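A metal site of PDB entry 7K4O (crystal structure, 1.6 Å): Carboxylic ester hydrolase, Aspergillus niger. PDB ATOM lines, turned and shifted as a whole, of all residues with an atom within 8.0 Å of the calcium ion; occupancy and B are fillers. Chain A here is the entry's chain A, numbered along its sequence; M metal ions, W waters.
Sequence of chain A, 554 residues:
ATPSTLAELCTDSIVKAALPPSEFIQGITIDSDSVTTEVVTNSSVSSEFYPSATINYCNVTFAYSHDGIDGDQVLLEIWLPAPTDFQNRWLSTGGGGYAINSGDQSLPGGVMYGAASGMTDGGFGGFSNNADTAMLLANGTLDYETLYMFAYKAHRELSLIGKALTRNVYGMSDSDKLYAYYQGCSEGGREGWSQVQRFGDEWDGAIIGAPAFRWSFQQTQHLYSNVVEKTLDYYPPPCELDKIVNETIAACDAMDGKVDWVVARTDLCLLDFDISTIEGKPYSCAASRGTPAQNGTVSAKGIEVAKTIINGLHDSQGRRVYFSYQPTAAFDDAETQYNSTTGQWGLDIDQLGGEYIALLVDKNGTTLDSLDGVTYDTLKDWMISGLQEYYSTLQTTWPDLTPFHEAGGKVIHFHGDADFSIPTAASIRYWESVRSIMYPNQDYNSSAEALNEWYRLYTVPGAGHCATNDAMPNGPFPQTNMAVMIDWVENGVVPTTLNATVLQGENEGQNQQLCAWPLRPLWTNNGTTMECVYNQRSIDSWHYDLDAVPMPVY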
ATOM      1  N   ILE A 249     -10.627  24.550   3.857  1.00  0.00           N
ATOM      2  CA  ILE A 249     -10.710  24.317   2.384  1.00  0.00           C
ATOM      3  C   ILE A 249     -10.133  22.927   2.091  1.00  0.00           C
ATOM      4  O   ILE A 249     -10.771  22.113   1.374  1.00  0.00           O
ATOM      5  CB  ILE A 249      -9.997  25.420   1.592  1.00  0.00           C
ATOM      6  CG1 ILE A 249     -10.749  26.750   1.691  1.00  0.00           C
ATOM      7  CG2 ILE A 249      -9.820  24.970   0.155  1.00  0.00           C
ATOM      8  CD1 ILE A 249      -9.968  27.940   1.202  1.00  0.00           C
ATOM      9  N   CYS A 252     -12.569  20.119   3.179  1.00  0.00           N
ATOM     10  CA  CYS A 252     -13.976  20.115   2.680  1.00  0.00           C
ATOM     11  C   CYS A 252     -13.999  20.129   1.153  1.00  0.00           C
ATOM     12  O   CYS A 252     -15.074  19.865   0.600  1.00  0.00           O
ATOM     13  CB  CYS A 252     -14.737  21.300   3.264  1.00  0.00           C
ATOM     14  SG  CYS A 252     -14.955  21.180   5.064  1.00  0.00           S
ATOM     15  N   ASP A 253     -12.848  20.347   0.502  1.00  0.00           N
ATOM     16  CA  ASP A 253     -12.733  20.357  -0.986  1.00  0.00           C
ATOM     17  C   ASP A 253     -13.455  19.162  -1.606  1.00  0.00           C
ATOM     18  O   ASP A 253     -14.308  19.372  -2.535  1.00  0.00           O
ATOM     19  CB  ASP A 253     -11.297  20.421  -1.402  1.00  0.00           C
ATOM     20  CG  ASP A 253     -11.086  20.372  -2.903  1.00  0.00           C
ATOM     21  OD1 ASP A 253     -12.047  20.659  -3.670  1.00  0.00           O
ATOM     22  OD2 ASP A 253      -9.928  20.076  -3.302  1.00  0.00           O
ATOM     23  N   ALA A 254     -13.144  17.951  -1.133  1.00  0.00           N
ATOM     24  CA  ALA A 254     -13.570  16.681  -1.768  1.00  0.00           C
ATOM     25  C   ALA A 254     -15.016  16.344  -1.412  1.00  0.00           C
ATOM     26  O   ALA A 254     -15.581  15.421  -1.986  1.00  0.00           O
ATOM     27  CB  ALA A 254     -12.628  15.560  -1.361  1.00  0.00           C
ATOM     28  N   MET A 255     -15.643  17.044  -0.490  1.00  0.00           N
ATOM     29  CA  MET A 255     -17.041  16.700  -0.109  1.00  0.00           C
ATOM     30  C   MET A 255     -18.043  16.977  -1.258  1.00  0.00           C
ATOM     31  O   MET A 255     -19.148  16.385  -1.248  1.00  0.00           O
ATOM     32  CB  MET A 255     -17.462  17.506   1.121  1.00  0.00           C
ATOM     33  CG  MET A 255     -16.784  17.039   2.406  1.00  0.00           C
ATOM     34  SD  MET A 255     -17.215  18.228   3.732  1.00  0.00           S
ATOM     35  CE  MET A 255     -16.251  17.630   5.131  1.00  0.00           C
ATOM     36  N   ASP A 256     -17.657  17.782  -2.230  1.00  0.00           N
ATOM     37  CA  ASP A 256     -18.490  18.052  -3.431  1.00  0.00           C
ATOM     38  C   ASP A 256     -18.215  17.026  -4.554  1.00  0.00           C
ATOM     39  O   ASP A 256     -18.859  17.118  -5.619  1.00  0.00           O
ATOM     40  CB  ASP A 256     -18.272  19.491  -3.913  1.00  0.00           C
ATOM     41  CG  ASP A 256     -16.843  19.910  -4.135  1.00  0.00           C
ATOM     42  OD1 ASP A 256     -16.090  19.154  -4.809  1.00  0.00           O
ATOM     43  OD2 ASP A 256     -16.493  21.012  -3.672  1.00  0.00           O
ATOM     44  N   GLY A 257     -17.308  16.059  -4.330  1.00  0.00           N
ATOM     45  CA  GLY A 257     -17.002  14.985  -5.302  1.00  0.00           C
ATOM     46  C   GLY A 257     -15.958  15.398  -6.317  1.00  0.00           C
ATOM     47  O   GLY A 257     -15.625  14.592  -7.234  1.00  0.00           O
ATOM     48  N   LYS A 258     -15.418  16.595  -6.192  1.00  0.00           N
ATOM     49  CA  LYS A 258     -14.433  17.117  -7.156  1.00  0.00           C
ATOM     50  C   LYS A 258     -13.263  17.708  -6.387  1.00  0.00           C
ATOM     51  O   LYS A 258     -13.446  18.669  -5.649  1.00  0.00           O
ATOM     52  CB  LYS A 258     -15.035  18.132  -8.119  1.00  0.00           C
ATOM     53  CG  LYS A 258     -14.069  18.511  -9.229  1.00  0.00           C
ATOM     54  CD  LYS A 258     -14.604  19.412 -10.301  1.00  0.00           C
ATOM     55  CE  LYS A 258     -13.637  19.441 -11.460  1.00  0.00           C
ATOM     56  NZ  LYS A 258     -13.850  20.620 -12.294  1.00  0.00           N
ATOM     57  N   VAL A 259     -12.071  17.172  -6.618  1.00  0.00           N
ATOM     58  CA  VAL A 259     -10.841  17.706  -5.978  1.00  0.00           C
ATOM     59  C   VAL A 259     -10.300  18.796  -6.878  1.00  0.00           C
ATOM     60  O   VAL A 259      -9.686  18.491  -7.915  1.00  0.00           O
ATOM     61  CB  VAL A 259      -9.819  16.580  -5.679  1.00  0.00           C
ATOM     62  CG1 VAL A 259      -8.508  17.157  -5.213  1.00  0.00           C
ATOM     63  CG2 VAL A 259     -10.382  15.608  -4.673  1.00  0.00           C
ATOM     64  N   ASP A 260     -10.523  20.047  -6.493  1.00  0.00           N
ATOM     65  CA  ASP A 260     -10.195  21.225  -7.324  1.00  0.00           C
ATOM     66  C   ASP A 260      -9.824  22.414  -6.445  1.00  0.00           C
ATOM     67  O   ASP A 260      -9.621  23.501  -6.987  1.00  0.00           O
ATOM     68  CB  ASP A 260     -11.385  21.554  -8.248  1.00  0.00           C
ATOM     69  CG  ASP A 260     -12.699  21.821  -7.508  1.00  0.00           C
ATOM     70  OD1 ASP A 260     -12.741  21.655  -6.267  1.00  0.00           O
ATOM     71  OD2 ASP A 260     -13.720  22.144  -8.211  1.00  0.00           O
ATOM     72  N   TRP A 261      -9.594  22.213  -5.146  1.00  0.00           N
ATOM     73  CA  TRP A 261      -9.361  23.331  -4.197  1.00  0.00           C
ATOM     74  C   TRP A 261     -10.523  24.370  -4.323  1.00  0.00           C
ATOM     75  O   TRP A 261     -10.272  25.559  -4.401  1.00  0.00           O
ATOM     76  CB  TRP A 261      -7.989  23.941  -4.431  1.00  0.00           C
ATOM     77  CG  TRP A 261      -7.507  24.679  -3.218  1.00  0.00           C
ATOM     78  CD1 TRP A 261      -7.465  26.034  -3.044  1.00  0.00           C
ATOM     79  CD2 TRP A 261      -7.057  24.087  -1.986  1.00  0.00           C
ATOM     80  NE1 TRP A 261      -6.994  26.324  -1.790  1.00  0.00           N
ATOM     81  CE2 TRP A 261      -6.728  25.160  -1.119  1.00  0.00           C
ATOM     82  CE3 TRP A 261      -6.826  22.768  -1.562  1.00  0.00           C
ATOM     83  CZ2 TRP A 261      -6.210  24.959   0.163  1.00  0.00           C
ATOM     84  CZ3 TRP A 261      -6.318  22.573  -0.287  1.00  0.00           C
ATOM     85  CH2 TRP A 261      -6.027  23.650   0.553  1.00  0.00           C
ATOM     86  N   VAL A 262     -11.729  23.847  -4.383  1.00  0.00           N
ATOM     87  CA  VAL A 262     -12.967  24.667  -4.333  1.00  0.00           C
ATOM     88  C   VAL A 262     -13.922  23.929  -3.441  1.00  0.00           C
ATOM     89  O   VAL A 262     -14.235  22.785  -3.686  1.00  0.00           O
ATOM     90  CB  VAL A 262     -13.575  24.902  -5.723  1.00  0.00           C
ATOM     91  CG1 VAL A 262     -14.790  25.836  -5.605  1.00  0.00           C
ATOM     92  CG2 VAL A 262     -12.551  25.478  -6.689  1.00  0.00           C
ATOM     93  N   VAL A 263     -14.459  24.620  -2.445  1.00  0.00           N
ATOM     94  CA  VAL A 263     -15.549  24.046  -1.624  1.00  0.00           C
ATOM     95  C   VAL A 263     -16.901  24.498  -2.175  1.00  0.00           C
ATOM     96  O   VAL A 263     -17.335  25.625  -1.865  1.00  0.00           O
ATOM     97  CB  VAL A 263     -15.333  24.458  -0.163  1.00  0.00           C
ATOM     98  CG1 VAL A 263     -16.464  23.951   0.712  1.00  0.00           C
ATOM     99  CG2 VAL A 263     -13.962  23.958   0.311  1.00  0.00           C
ATOM    100  N   ALA A 264     -17.547  23.618  -2.919  1.00  0.00           N
ATOM    101  CA  ALA A 264     -18.890  23.853  -3.487  1.00  0.00           C
ATOM    102  C   ALA A 264     -19.939  23.451  -2.466  1.00  0.00           C
ATOM    103  O   ALA A 264     -21.108  23.723  -2.718  1.00  0.00           O
ATOM    104  CB  ALA A 264     -19.074  23.081  -4.764  1.00  0.00           C
ATOM    105  N   ARG A 265     -19.574  22.699  -1.412  1.00  0.00           N
ATOM    106  CA  ARG A 265     -20.560  22.247  -0.419  1.00  0.00           C
ATOM    107  C   ARG A 265     -20.111  22.741   0.956  1.00  0.00           C
ATOM    108  O   ARG A 265     -19.663  21.926   1.811  1.00  0.00           O
ATOM    109  CB  ARG A 265     -20.770  20.726  -0.517  1.00  0.00           C
ATOM    110  CG  ARG A 265     -21.394  20.324  -1.846  1.00  0.00           C
ATOM    111  CD  ARG A 265     -22.865  20.695  -1.962  1.00  0.00           C
ATOM    112  NE  ARG A 265     -23.700  19.979  -1.051  1.00  0.00           N
ATOM    113  CZ  ARG A 265     -24.190  18.763  -1.211  1.00  0.00           C
ATOM    114  NH1 ARG A 265     -23.979  18.104  -2.348  1.00  0.00           N
ATOM    115  NH2 ARG A 265     -24.921  18.211  -0.273  1.00  0.00           N
ATOM    116  N   PRO A 461     -19.698  28.433  -5.902  1.00  0.00           N
ATOM    117  CA  PRO A 461     -18.587  27.730  -5.237  1.00  0.00           C
ATOM    118  C   PRO A 461     -17.315  28.539  -5.127  1.00  0.00           C
ATOM    119  O   PRO A 461     -16.837  29.125  -6.081  1.00  0.00           O
ATOM    120  CB  PRO A 461     -18.340  26.491  -6.132  1.00  0.00           C
ATOM    121  CG  PRO A 461     -19.680  26.208  -6.732  1.00  0.00           C
ATOM    122  CD  PRO A 461     -20.322  27.596  -6.936  1.00  0.00           C
ATOM    123  N   MET A 472      -9.364  30.443  -3.847  1.00  0.00           N
ATOM    124  CA  MET A 472     -10.015  29.336  -4.567  1.00  0.00           C
ATOM    125  C   MET A 472     -10.166  29.761  -6.029  1.00  0.00           C
ATOM    126  O   MET A 472     -11.278  29.887  -6.566  1.00  0.00           O
ATOM    127  CB  MET A 472     -11.330  28.891  -3.920  1.00  0.00           C
ATOM    128  CG  MET A 472     -11.128  28.240  -2.558  1.00  0.00           C
ATOM    129  SD  MET A 472     -12.561  27.587  -1.747  1.00  0.00           S
ATOM    130  CE  MET A 472     -13.078  29.063  -0.869  1.00  0.00           C
ATOM    131  N   TRP A 523     -20.417  16.262  -7.737  1.00  0.00           N
ATOM    132  CA  TRP A 523     -19.713  15.686  -8.919  1.00  0.00           C
ATOM    133  C   TRP A 523     -19.548  14.171  -8.723  1.00  0.00           C
ATOM    134  O   TRP A 523     -19.276  13.726  -7.586  1.00  0.00           O
ATOM    135  CB  TRP A 523     -18.381  16.357  -9.178  1.00  0.00           C
ATOM    136  CG  TRP A 523     -18.456  17.840  -9.450  1.00  0.00           C
ATOM    137  CD1 TRP A 523     -18.670  18.836  -8.530  1.00  0.00           C
ATOM    138  CD2 TRP A 523     -18.222  18.512 -10.692  1.00  0.00           C
ATOM    139  NE1 TRP A 523     -18.602  20.067  -9.118  1.00  0.00           N
ATOM    140  CE2 TRP A 523     -18.347  19.903 -10.454  1.00  0.00           C
ATOM    141  CE3 TRP A 523     -17.960  18.090 -11.996  1.00  0.00           C
ATOM    142  CZ2 TRP A 523     -18.215  20.855 -11.471  1.00  0.00           C
ATOM    143  CZ3 TRP A 523     -17.820  19.023 -13.000  1.00  0.00           C
ATOM    144  CH2 TRP A 523     -17.956  20.400 -12.744  1.00  0.00           C
HETATM  145 CA    CA M   1     -14.284  20.588  -4.607  1.00  0.00          CA
HETATM  146  O   HOH W   1     -15.705  21.578  -6.527  1.00  0.00           O
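The backbone NH (N) of Ala 264 lies close to the side-chain carboxylate (OD2) of Asp 256 (2.9 Å). The backbone carbonyl oxygen (O) of Asp 256 is in hydrogen-bond range of the backbone NH (N) of Trp 523 (2.8 Å). The side-chain carboxylate (OD2) of Asp 253 lies within hydrogen-bond range of the backbone NH (N) of Trp 261 (2.8 Å).
The calcium ion is bound by the side-chain carboxylate (OD1) of Asp 256 (2.3 Å), the backbone carbonyl oxygen (O) of Lys 258 (2.3 Å), the backbone carbonyl oxygen (O) of Val 262 (2.4 Å), the backbone carbonyl oxygen (O) of Asp 253 (2.4 Å), the side-chain carboxylate (OD1) of Asp 253 (2.4 Å), the side-chain carboxylate (OD2) of Asp 256 (2.4 Å), the side-chain carboxylate (OD1) of Asp 260 (2.5 Å) and water W1 (2.6 Å).
Within 4 Å of the calcium ion: Asp 253, Asp 256, Lys 258, Asp 260 and Val 262.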
